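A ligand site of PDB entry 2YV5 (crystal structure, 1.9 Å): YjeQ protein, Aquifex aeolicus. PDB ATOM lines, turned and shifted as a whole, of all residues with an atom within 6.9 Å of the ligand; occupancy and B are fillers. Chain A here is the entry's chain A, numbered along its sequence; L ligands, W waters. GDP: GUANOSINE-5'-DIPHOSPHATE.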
ATOM      1  N   VAL A  86      14.203 -16.831 -29.524  1.00  0.00           N
ATOM      2  CA  VAL A  86      15.076 -16.281 -28.499  1.00  0.00           C
ATOM      3  C   VAL A  86      14.726 -14.812 -28.278  1.00  0.00           C
ATOM      4  O   VAL A  86      14.568 -14.034 -29.236  1.00  0.00           O
ATOM      5  CB  VAL A  86      16.555 -16.423 -28.909  1.00  0.00           C
ATOM      6  CG1 VAL A  86      17.473 -16.038 -27.739  1.00  0.00           C
ATOM      7  CG2 VAL A  86      16.820 -17.888 -29.350  1.00  0.00           C
ATOM      8  N   MET A  91      18.884  -5.641 -23.616  1.00  0.00           N
ATOM      9  CA  MET A  91      20.044  -5.880 -24.480  1.00  0.00           C
ATOM     10  C   MET A  91      19.851  -7.014 -25.496  1.00  0.00           C
ATOM     11  O   MET A  91      20.579  -8.022 -25.491  1.00  0.00           O
ATOM     12  CB  MET A  91      21.278  -6.174 -23.610  1.00  0.00           C
ATOM     13  CG  MET A  91      22.583  -5.714 -24.219  1.00  0.00           C
ATOM     14  SD  MET A  91      23.936  -5.935 -23.053  1.00  0.00           S
ATOM     15  CE  MET A  91      23.374  -4.908 -21.719  1.00  0.00           C
ATOM     16  N   ASN A 118      16.822 -15.431 -22.969  1.00  0.00           N
ATOM     17  CA  ASN A 118      18.272 -15.544 -22.742  1.00  0.00           C
ATOM     18  C   ASN A 118      18.796 -14.330 -21.961  1.00  0.00           C
ATOM     19  O   ASN A 118      18.039 -13.389 -21.674  1.00  0.00           O
ATOM     20  CB  ASN A 118      18.958 -15.636 -24.125  1.00  0.00           C
ATOM     21  CG  ASN A 118      20.444 -15.931 -24.035  1.00  0.00           C
ATOM     22  OD1 ASN A 118      20.885 -16.698 -23.197  1.00  0.00           O
ATOM     23  ND2 ASN A 118      21.225 -15.329 -24.935  1.00  0.00           N
ATOM     24  N   LYS A 119      20.085 -14.366 -21.605  1.00  0.00           N
ATOM     25  CA  LYS A 119      20.746 -13.282 -20.898  1.00  0.00           C
ATOM     26  C   LYS A 119      20.177 -12.978 -19.512  1.00  0.00           C
ATOM     27  O   LYS A 119      20.250 -11.848 -19.048  1.00  0.00           O
ATOM     28  CB  LYS A 119      20.700 -12.008 -21.750  1.00  0.00           C
ATOM     29  CG  LYS A 119      21.315 -12.180 -23.137  1.00  0.00           C
ATOM     30  CD  LYS A 119      21.736 -10.812 -23.695  1.00  0.00           C
ATOM     31  CE  LYS A 119      22.187 -10.901 -25.167  1.00  0.00           C
ATOM     32  NZ  LYS A 119      22.709  -9.587 -25.678  1.00  0.00           N
ATOM     33  N   ILE A 120      19.640 -13.999 -18.848  1.00  0.00           N
ATOM     34  CA  ILE A 120      19.071 -13.811 -17.513  1.00  0.00           C
ATOM     35  C   ILE A 120      20.170 -13.433 -16.501  1.00  0.00           C
ATOM     36  O   ILE A 120      19.883 -12.901 -15.430  1.00  0.00           O
ATOM     37  CB  ILE A 120      18.342 -15.098 -17.015  1.00  0.00           C
ATOM     38  CG1 ILE A 120      19.301 -16.287 -16.980  1.00  0.00           C
ATOM     39  CG2 ILE A 120      17.154 -15.402 -17.919  1.00  0.00           C
ATOM     40  CD1 ILE A 120      18.652 -17.611 -16.557  1.00  0.00           C
ATOM     41  N   ASP A 121      21.410 -13.715 -16.864  1.00  0.00           N
ATOM     42  CA  ASP A 121      22.530 -13.396 -15.981  1.00  0.00           C
ATOM     43  C   ASP A 121      22.723 -11.871 -15.826  1.00  0.00           C
ATOM     44  O   ASP A 121      23.392 -11.421 -14.885  1.00  0.00           O
ATOM     45  CB  ASP A 121      23.805 -14.013 -16.534  1.00  0.00           C
ATOM     46  CG  ASP A 121      24.136 -13.530 -17.932  1.00  0.00           C
ATOM     47  OD1 ASP A 121      23.532 -14.024 -18.897  1.00  0.00           O
ATOM     48  OD2 ASP A 121      25.005 -12.631 -18.084  1.00  0.00           O
ATOM     49  N   LEU A 122      22.152 -11.099 -16.741  1.00  0.00           N
ATOM     50  CA  LEU A 122      22.293  -9.630 -16.693  1.00  0.00           C
ATOM     51  C   LEU A 122      21.243  -8.909 -15.849  1.00  0.00           C
ATOM     52  O   LEU A 122      21.383  -7.718 -15.549  1.00  0.00           O
ATOM     53  CB  LEU A 122      22.202  -9.058 -18.113  1.00  0.00           C
ATOM     54  CG  LEU A 122      23.301  -9.396 -19.114  1.00  0.00           C
ATOM     55  CD1 LEU A 122      23.002  -8.706 -20.452  1.00  0.00           C
ATOM     56  CD2 LEU A 122      24.658  -8.948 -18.571  1.00  0.00           C
ATOM     57  N   VAL A 148      17.212 -19.076 -19.982  1.00  0.00           N
ATOM     58  CA  VAL A 148      18.594 -19.582 -20.066  1.00  0.00           C
ATOM     59  C   VAL A 148      19.601 -18.449 -20.062  1.00  0.00           C
ATOM     60  O   VAL A 148      19.255 -17.279 -20.227  1.00  0.00           O
ATOM     61  CB  VAL A 148      18.908 -20.363 -21.388  1.00  0.00           C
ATOM     62  CG1 VAL A 148      17.961 -21.556 -21.572  1.00  0.00           C
ATOM     63  CG2 VAL A 148      18.799 -19.403 -22.595  1.00  0.00           C
ATOM     64  N   SER A 149      20.855 -18.820 -19.838  1.00  0.00           N
ATOM     65  CA  SER A 149      21.938 -17.862 -19.950  1.00  0.00           C
ATOM     66  C   SER A 149      22.966 -18.611 -20.784  1.00  0.00           C
ATOM     67  O   SER A 149      23.569 -19.567 -20.291  1.00  0.00           O
ATOM     68  CB  SER A 149      22.582 -17.510 -18.614  1.00  0.00           C
ATOM     69  OG  SER A 149      23.732 -16.703 -18.875  1.00  0.00           O
ATOM     70  N   ALA A 150      23.122 -18.216 -22.047  1.00  0.00           N
ATOM     71  CA  ALA A 150      24.118 -18.857 -22.891  1.00  0.00           C
ATOM     72  C   ALA A 150      25.512 -18.538 -22.341  1.00  0.00           C
ATOM     73  O   ALA A 150      26.475 -19.279 -22.569  1.00  0.00           O
ATOM     74  CB  ALA A 150      23.998 -18.370 -24.331  1.00  0.00           C
ATOM     75  N   LYS A 151      25.616 -17.430 -21.605  1.00  0.00           N
ATOM     76  CA  LYS A 151      26.910 -17.050 -21.046  1.00  0.00           C
ATOM     77  C   LYS A 151      27.366 -17.961 -19.922  1.00  0.00           C
ATOM     78  O   LYS A 151      28.489 -18.463 -19.944  1.00  0.00           O
ATOM     79  CB  LYS A 151      26.896 -15.607 -20.522  1.00  0.00           C
ATOM     80  CG  LYS A 151      28.190 -15.227 -19.756  1.00  0.00           C
ATOM     81  CD  LYS A 151      28.193 -13.750 -19.315  1.00  0.00           C
ATOM     82  CE  LYS A 151      29.337 -13.460 -18.344  1.00  0.00           C
ATOM     83  NZ  LYS A 151      29.691 -12.014 -18.333  1.00  0.00           N
ATOM     84  N   THR A 152      26.503 -18.192 -18.933  1.00  0.00           N
ATOM     85  CA  THR A 152      26.869 -19.048 -17.821  1.00  0.00           C
ATOM     86  C   THR A 152      26.559 -20.519 -18.121  1.00  0.00           C
ATOM     87  O   THR A 152      27.159 -21.405 -17.508  1.00  0.00           O
ATOM     88  CB  THR A 152      26.097 -18.674 -16.545  1.00  0.00           C
ATOM     89  OG1 THR A 152      24.709 -19.052 -16.676  1.00  0.00           O
ATOM     90  CG2 THR A 152      26.226 -17.192 -16.264  1.00  0.00           C
ATOM     91  N   GLY A 153      25.644 -20.760 -19.052  1.00  0.00           N
ATOM     92  CA  GLY A 153      25.222 -22.105 -19.393  1.00  0.00           C
ATOM     93  C   GLY A 153      23.968 -22.533 -18.618  1.00  0.00           C
ATOM     94  O   GLY A 153      23.396 -23.595 -18.880  1.00  0.00           O
ATOM     95  N   ALA A 171      15.014 -18.396 -33.927  1.00  0.00           N
ATOM     96  CA  ALA A 171      14.472 -17.153 -34.460  1.00  0.00           C
ATOM     97  C   ALA A 171      14.586 -16.092 -33.363  1.00  0.00           C
ATOM     98  O   ALA A 171      14.957 -16.420 -32.231  1.00  0.00           O
ATOM     99  CB  ALA A 171      12.982 -17.341 -34.909  1.00  0.00           C
ATOM    100  N   GLY A 172      14.271 -14.844 -33.709  1.00  0.00           N
ATOM    101  CA  GLY A 172      14.343 -13.765 -32.741  1.00  0.00           C
ATOM    102  C   GLY A 172      15.139 -12.612 -33.297  1.00  0.00           C
ATOM    103  O   GLY A 172      15.942 -12.813 -34.215  1.00  0.00           O
ATOM    104  N   PRO A 173      14.976 -11.410 -32.751  1.00  0.00           N
ATOM    105  CA  PRO A 173      15.694 -10.228 -33.237  1.00  0.00           C
ATOM    106  C   PRO A 173      17.193 -10.227 -33.052  1.00  0.00           C
ATOM    107  O   PRO A 173      17.746 -10.987 -32.238  1.00  0.00           O
ATOM    108  CB  PRO A 173      15.016  -9.082 -32.490  1.00  0.00           C
ATOM    109  CG  PRO A 173      14.673  -9.716 -31.154  1.00  0.00           C
ATOM    110  CD  PRO A 173      14.154 -11.096 -31.560  1.00  0.00           C
ATOM    111  N   SER A 174      17.884  -9.353 -33.781  1.00  0.00           N
ATOM    112  CA  SER A 174      19.335  -9.305 -33.650  1.00  0.00           C
ATOM    113  C   SER A 174      19.833  -9.009 -32.227  1.00  0.00           C
ATOM    114  O   SER A 174      19.310  -8.119 -31.525  1.00  0.00           O
ATOM    115  CB  SER A 174      19.877  -8.249 -34.624  1.00  0.00           C
ATOM    116  OG  SER A 174      21.256  -8.046 -34.431  1.00  0.00           O
ATOM    117  N   GLY A 175      20.851  -9.754 -31.800  1.00  0.00           N
ATOM    118  CA  GLY A 175      21.489  -9.535 -30.513  1.00  0.00           C
ATOM    119  C   GLY A 175      20.975 -10.286 -29.310  1.00  0.00           C
ATOM    120  O   GLY A 175      21.540 -10.139 -28.227  1.00  0.00           O
ATOM    121  N   VAL A 176      19.932 -11.106 -29.477  1.00  0.00           N
ATOM    122  CA  VAL A 176      19.391 -11.810 -28.322  1.00  0.00           C
ATOM    123  C   VAL A 176      20.245 -12.992 -27.865  1.00  0.00           C
ATOM    124  O   VAL A 176      20.115 -13.459 -26.730  1.00  0.00           O
ATOM    125  CB  VAL A 176      17.949 -12.313 -28.587  1.00  0.00           C
ATOM    126  CG1 VAL A 176      17.011 -11.109 -28.745  1.00  0.00           C
ATOM    127  CG2 VAL A 176      17.928 -13.188 -29.877  1.00  0.00           C
ATOM    128  N   GLY A 177      21.108 -13.471 -28.768  1.00  0.00           N
ATOM    129  CA  GLY A 177      21.952 -14.601 -28.424  1.00  0.00           C
ATOM    130  C   GLY A 177      21.683 -15.870 -29.239  1.00  0.00           C
ATOM    131  O   GLY A 177      22.037 -16.948 -28.785  1.00  0.00           O
ATOM    132  N   LYS A 178      21.081 -15.764 -30.427  1.00  0.00           N
ATOM    133  CA  LYS A 178      20.817 -16.976 -31.213  1.00  0.00           C
ATOM    134  C   LYS A 178      22.104 -17.737 -31.545  1.00  0.00           C
ATOM    135  O   LYS A 178      22.170 -18.956 -31.418  1.00  0.00           O
ATOM    136  CB  LYS A 178      20.071 -16.645 -32.524  1.00  0.00           C
ATOM    137  CG  LYS A 178      18.698 -15.969 -32.338  1.00  0.00           C
ATOM    138  CD  LYS A 178      18.057 -15.613 -33.710  1.00  0.00           C
ATOM    139  CE  LYS A 178      18.910 -14.636 -34.546  1.00  0.00           C
ATOM    140  NZ  LYS A 178      18.941 -13.267 -33.951  1.00  0.00           N
ATOM    141  N   SER A 179      23.132 -17.008 -31.986  1.00  0.00           N
ATOM    142  CA  SER A 179      24.394 -17.650 -32.323  1.00  0.00           C
ATOM    143  C   SER A 179      25.077 -18.245 -31.082  1.00  0.00           C
ATOM    144  O   SER A 179      25.658 -19.333 -31.151  1.00  0.00           O
ATOM    145  CB  SER A 179      25.314 -16.632 -33.030  1.00  0.00           C
ATOM    146  OG  SER A 179      26.382 -17.304 -33.673  1.00  0.00           O
ATOM    147  N   SER A 180      24.982 -17.539 -29.956  1.00  0.00           N
ATOM    148  CA  SER A 180      25.580 -18.015 -28.691  1.00  0.00           C
ATOM    149  C   SER A 180      24.899 -19.294 -28.237  1.00  0.00           C
ATOM    150  O   SER A 180      25.531 -20.201 -27.715  1.00  0.00           O
ATOM    151  CB  SER A 180      25.435 -16.957 -27.589  1.00  0.00           C
ATOM    152  OG  SER A 180      26.117 -15.774 -27.960  1.00  0.00           O
ATOM    153  N   ILE A 181      23.585 -19.358 -28.419  1.00  0.00           N
ATOM    154  CA  ILE A 181      22.878 -20.565 -28.058  1.00  0.00           C
ATOM    155  C   ILE A 181      23.228 -21.697 -29.028  1.00  0.00           C
ATOM    156  O   ILE A 181      23.428 -22.824 -28.608  1.00  0.00           O
ATOM    157  CB  ILE A 181      21.343 -20.292 -28.009  1.00  0.00           C
ATOM    158  CG1 ILE A 181      21.038 -19.452 -26.773  1.00  0.00           C
ATOM    159  CG2 ILE A 181      20.542 -21.625 -27.953  1.00  0.00           C
ATOM    160  CD1 ILE A 181      19.580 -18.889 -26.651  1.00  0.00           C
ATOM    161  N   LEU A 182      23.308 -21.411 -30.328  1.00  0.00           N
ATOM    162  CA  LEU A 182      23.658 -22.469 -31.292  1.00  0.00           C
ATOM    163  C   LEU A 182      25.062 -22.977 -30.956  1.00  0.00           C
ATOM    164  O   LEU A 182      25.341 -24.179 -31.056  1.00  0.00           O
ATOM    165  CB  LEU A 182      23.647 -21.927 -32.732  1.00  0.00           C
ATOM    166  CG  LEU A 182      24.008 -22.974 -33.832  1.00  0.00           C
ATOM    167  CD1 LEU A 182      22.931 -24.088 -33.881  1.00  0.00           C
ATOM    168  CD2 LEU A 182      24.117 -22.257 -35.209  1.00  0.00           C
ATOM    169  N   GLU A 189      28.611 -21.828 -35.577  1.00  0.00           N
ATOM    170  CA  GLU A 189      28.196 -20.443 -35.687  1.00  0.00           C
ATOM    171  C   GLU A 189      26.985 -20.310 -36.611  1.00  0.00           C
ATOM    172  O   GLU A 189      26.836 -21.049 -37.579  1.00  0.00           O
ATOM    173  CB  GLU A 189      29.351 -19.599 -36.243  1.00  0.00           C
ATOM    174  CG  GLU A 189      30.570 -19.506 -35.316  1.00  0.00           C
ATOM    175  CD  GLU A 189      30.395 -18.484 -34.195  1.00  0.00           C
ATOM    176  OE1 GLU A 189      29.412 -18.588 -33.425  1.00  0.00           O
ATOM    177  OE2 GLU A 189      31.244 -17.579 -34.091  1.00  0.00           O
ATOM    178  N   LEU A 190      26.108 -19.377 -36.270  1.00  0.00           N
ATOM    179  CA  LEU A 190      24.924 -19.134 -37.065  1.00  0.00           C
ATOM    180  C   LEU A 190      25.393 -18.459 -38.365  1.00  0.00           C
ATOM    181  O   LEU A 190      26.171 -17.499 -38.315  1.00  0.00           O
ATOM    182  CB  LEU A 190      23.992 -18.222 -36.287  1.00  0.00           C
ATOM    183  CG  LEU A 190      22.533 -18.144 -36.681  1.00  0.00           C
ATOM    184  CD1 LEU A 190      21.906 -19.513 -36.674  1.00  0.00           C
ATOM    185  CD2 LEU A 190      21.814 -17.215 -35.703  1.00  0.00           C
HETATM  186  PB  GDP L   1      22.272 -13.091 -32.205  1.00  0.00           P
HETATM  187  O1B GDP L   1      20.832 -13.317 -31.882  1.00  0.00           O
HETATM  188  O2B GDP L   1      22.475 -11.786 -33.115  1.00  0.00           O
HETATM  189  O3B GDP L   1      22.896 -14.346 -32.996  1.00  0.00           O
HETATM  190  O3A GDP L   1      23.125 -12.846 -30.854  1.00  0.00           O
HETATM  191  PA  GDP L   1      24.656 -13.302 -30.590  1.00  0.00           P
HETATM  192  O1A GDP L   1      25.534 -12.741 -31.651  1.00  0.00           O
HETATM  193  O2A GDP L   1      24.713 -14.754 -30.331  1.00  0.00           O
HETATM  194  O5' GDP L   1      24.926 -12.513 -29.203  1.00  0.00           O
HETATM  195  C5' GDP L   1      24.982 -11.083 -29.213  1.00  0.00           C
HETATM  196  C4' GDP L   1      25.774 -10.583 -28.009  1.00  0.00           C
HETATM  197  O4' GDP L   1      25.154 -11.076 -26.812  1.00  0.00           O
HETATM  198  C3' GDP L   1      27.175 -11.184 -28.055  1.00  0.00           C
HETATM  199  O3' GDP L   1      28.127 -10.245 -27.565  1.00  0.00           O
HETATM  200  C2' GDP L   1      27.051 -12.398 -27.135  1.00  0.00           C
HETATM  201  O2' GDP L   1      28.317 -12.675 -26.545  1.00  0.00           O
HETATM  202  C1' GDP L   1      26.135 -11.813 -26.058  1.00  0.00           C
HETATM  203  N9  GDP L   1      25.456 -12.861 -25.261  1.00  0.00           N
HETATM  204  C8  GDP L   1      24.859 -13.950 -25.769  1.00  0.00           C
HETATM  205  N7  GDP L   1      24.294 -14.633 -24.772  1.00  0.00           N
HETATM  206  C5  GDP L   1      24.531 -13.993 -23.645  1.00  0.00           C
HETATM  207  C6  GDP L   1      24.168 -14.233 -22.309  1.00  0.00           C
HETATM  208  O6  GDP L   1      23.496 -15.203 -21.982  1.00  0.00           O
HETATM  209  N1  GDP L   1      24.578 -13.314 -21.337  1.00  0.00           N
HETATM  210  C2  GDP L   1      25.320 -12.195 -21.710  1.00  0.00           C
HETATM  211  N2  GDP L   1      25.723 -11.334 -20.781  1.00  0.00           N
HETATM  212  N3  GDP L   1      25.644 -11.991 -22.998  1.00  0.00           N
HETATM  213  C4  GDP L   1      25.265 -12.868 -23.947  1.00  0.00           C
HETATM  214  O   HOH W   1      27.623  -8.303 -25.437  1.00  0.00           O
HETATM  215  O   HOH W   2      24.930  -8.835 -24.245  1.00  0.00           O
HETATM  216  O   HOH W   3      24.486  -9.947 -32.723  1.00  0.00           O
HETATM  217  O   HOH W   4      22.286 -11.204 -35.574  1.00  0.00           O
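CD2 of Leu 122 touches N2 of the ligand, at 3.4 Å. Pro 173 touches the ligand. C of Ser 174 touches O2B of the ligand, 3.9 Å away. Hydrophobic or aromatic side chains within 4 Å of the ligand: Leu 122, Ala 150 and Val 176. Within 4 Å of the ligand: Asn 118, Lys 119, Asp 121, Leu 122, Ser 149, Ala 150, Lys 151, Pro 173, Ser 174, Gly 175, Val 176, Gly 177, Lys 178, Ser 179 and Ser 180.
An oxygen (O3B) of the ligand is in hydrogen-bond range of the backbone NH (N) of Ser 179 (2.9 Å). A nitrogen (N7) of the ligand sits at hydrogen-bond distance from the side-chain amide nitrogen of Asn 118, 3.2 Å away. The backbone NH of Ser 180 sits at hydrogen-bond distance from an oxygen (O2A) of the ligand (2.8 Å). The backbone NH (N) of Lys 178 sits at hydrogen-bond distance from an oxygen (O1B) of the ligand (2.9 Å). The side-chain hydroxyl (OG) of Ser 149 is in hydrogen-bond range of an oxygen (O6) of the ligand, at 3.5 Å. An oxygen (O1B) of the ligand lies within salt-bridge range of the side-chain amino group of Lys 178. O6 of the ligand is in hydrogen-bond range of N of Ala 150. O3A of the ligand sits at hydrogen-bond distance from N of Gly 177, 3.0 Å away. The side-chain carboxylate (OD1) of Asp 121 is in hydrogen-bond range of a nitrogen (N1) of the ligand. An oxygen (O1B) of the ligand sits at hydrogen-bond distance from the backbone NH of Val 176 (3.4 Å). An oxygen (O6) of the ligand lies within hydrogen-bond range of the backbone NH (N) of Lys 151. The backbone NH of Gly 175 is in hydrogen-bond range of an oxygen (O2B) of the ligand, 2.9 Å away. The side-chain amino group of Lys 119 sits at hydrogen-bond distance from an oxygen (O4') of the ligand (3.1 Å). The side-chain hydroxyl (OG) of Ser 180 sits at hydrogen-bond distance from an oxygen (O2A) of the ligand (2.9 Å).
Water W2 lies within hydrogen-bond range of the side-chain amino group (NZ) of Lys 119 (2.7 Å), the side-chain sulfur (SD) of Met 91 (3.3 Å) and an oxygen (O4') of the ligand (3.4 Å).
The side-chain amino group (NZ) of Lys 178 sits at hydrogen-bond distance from the backbone carbonyl oxygen (O) of Gly 172 (3.0 Å). The side-chain amino group (NZ) of Lys 119 lies within hydrogen-bond range of the backbone carbonyl oxygen (O) of Gly 175, at 2.9 Å. The side-chain hydroxyl of Ser 149 sits at hydrogen-bond distance from the backbone NH of Thr 152 (3.1 Å). OD1 of Asp 121 sits at hydrogen-bond distance from OG of Ser 149 (2.7 Å). The backbone carbonyl oxygen (O) of Met 91 is in hydrogen-bond range of the side-chain amino group (NZ) of Lys 119, at 2.6 Å. N of Lys 151 lies close to OG of Ser 149, 3.4 Å away. N of Ala 150 lies within hydrogen-bond range of OD1 of Asn 118 (2.9 Å). N of Lys 119 sits at hydrogen-bond distance from O of Val 148 (3.3 Å).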
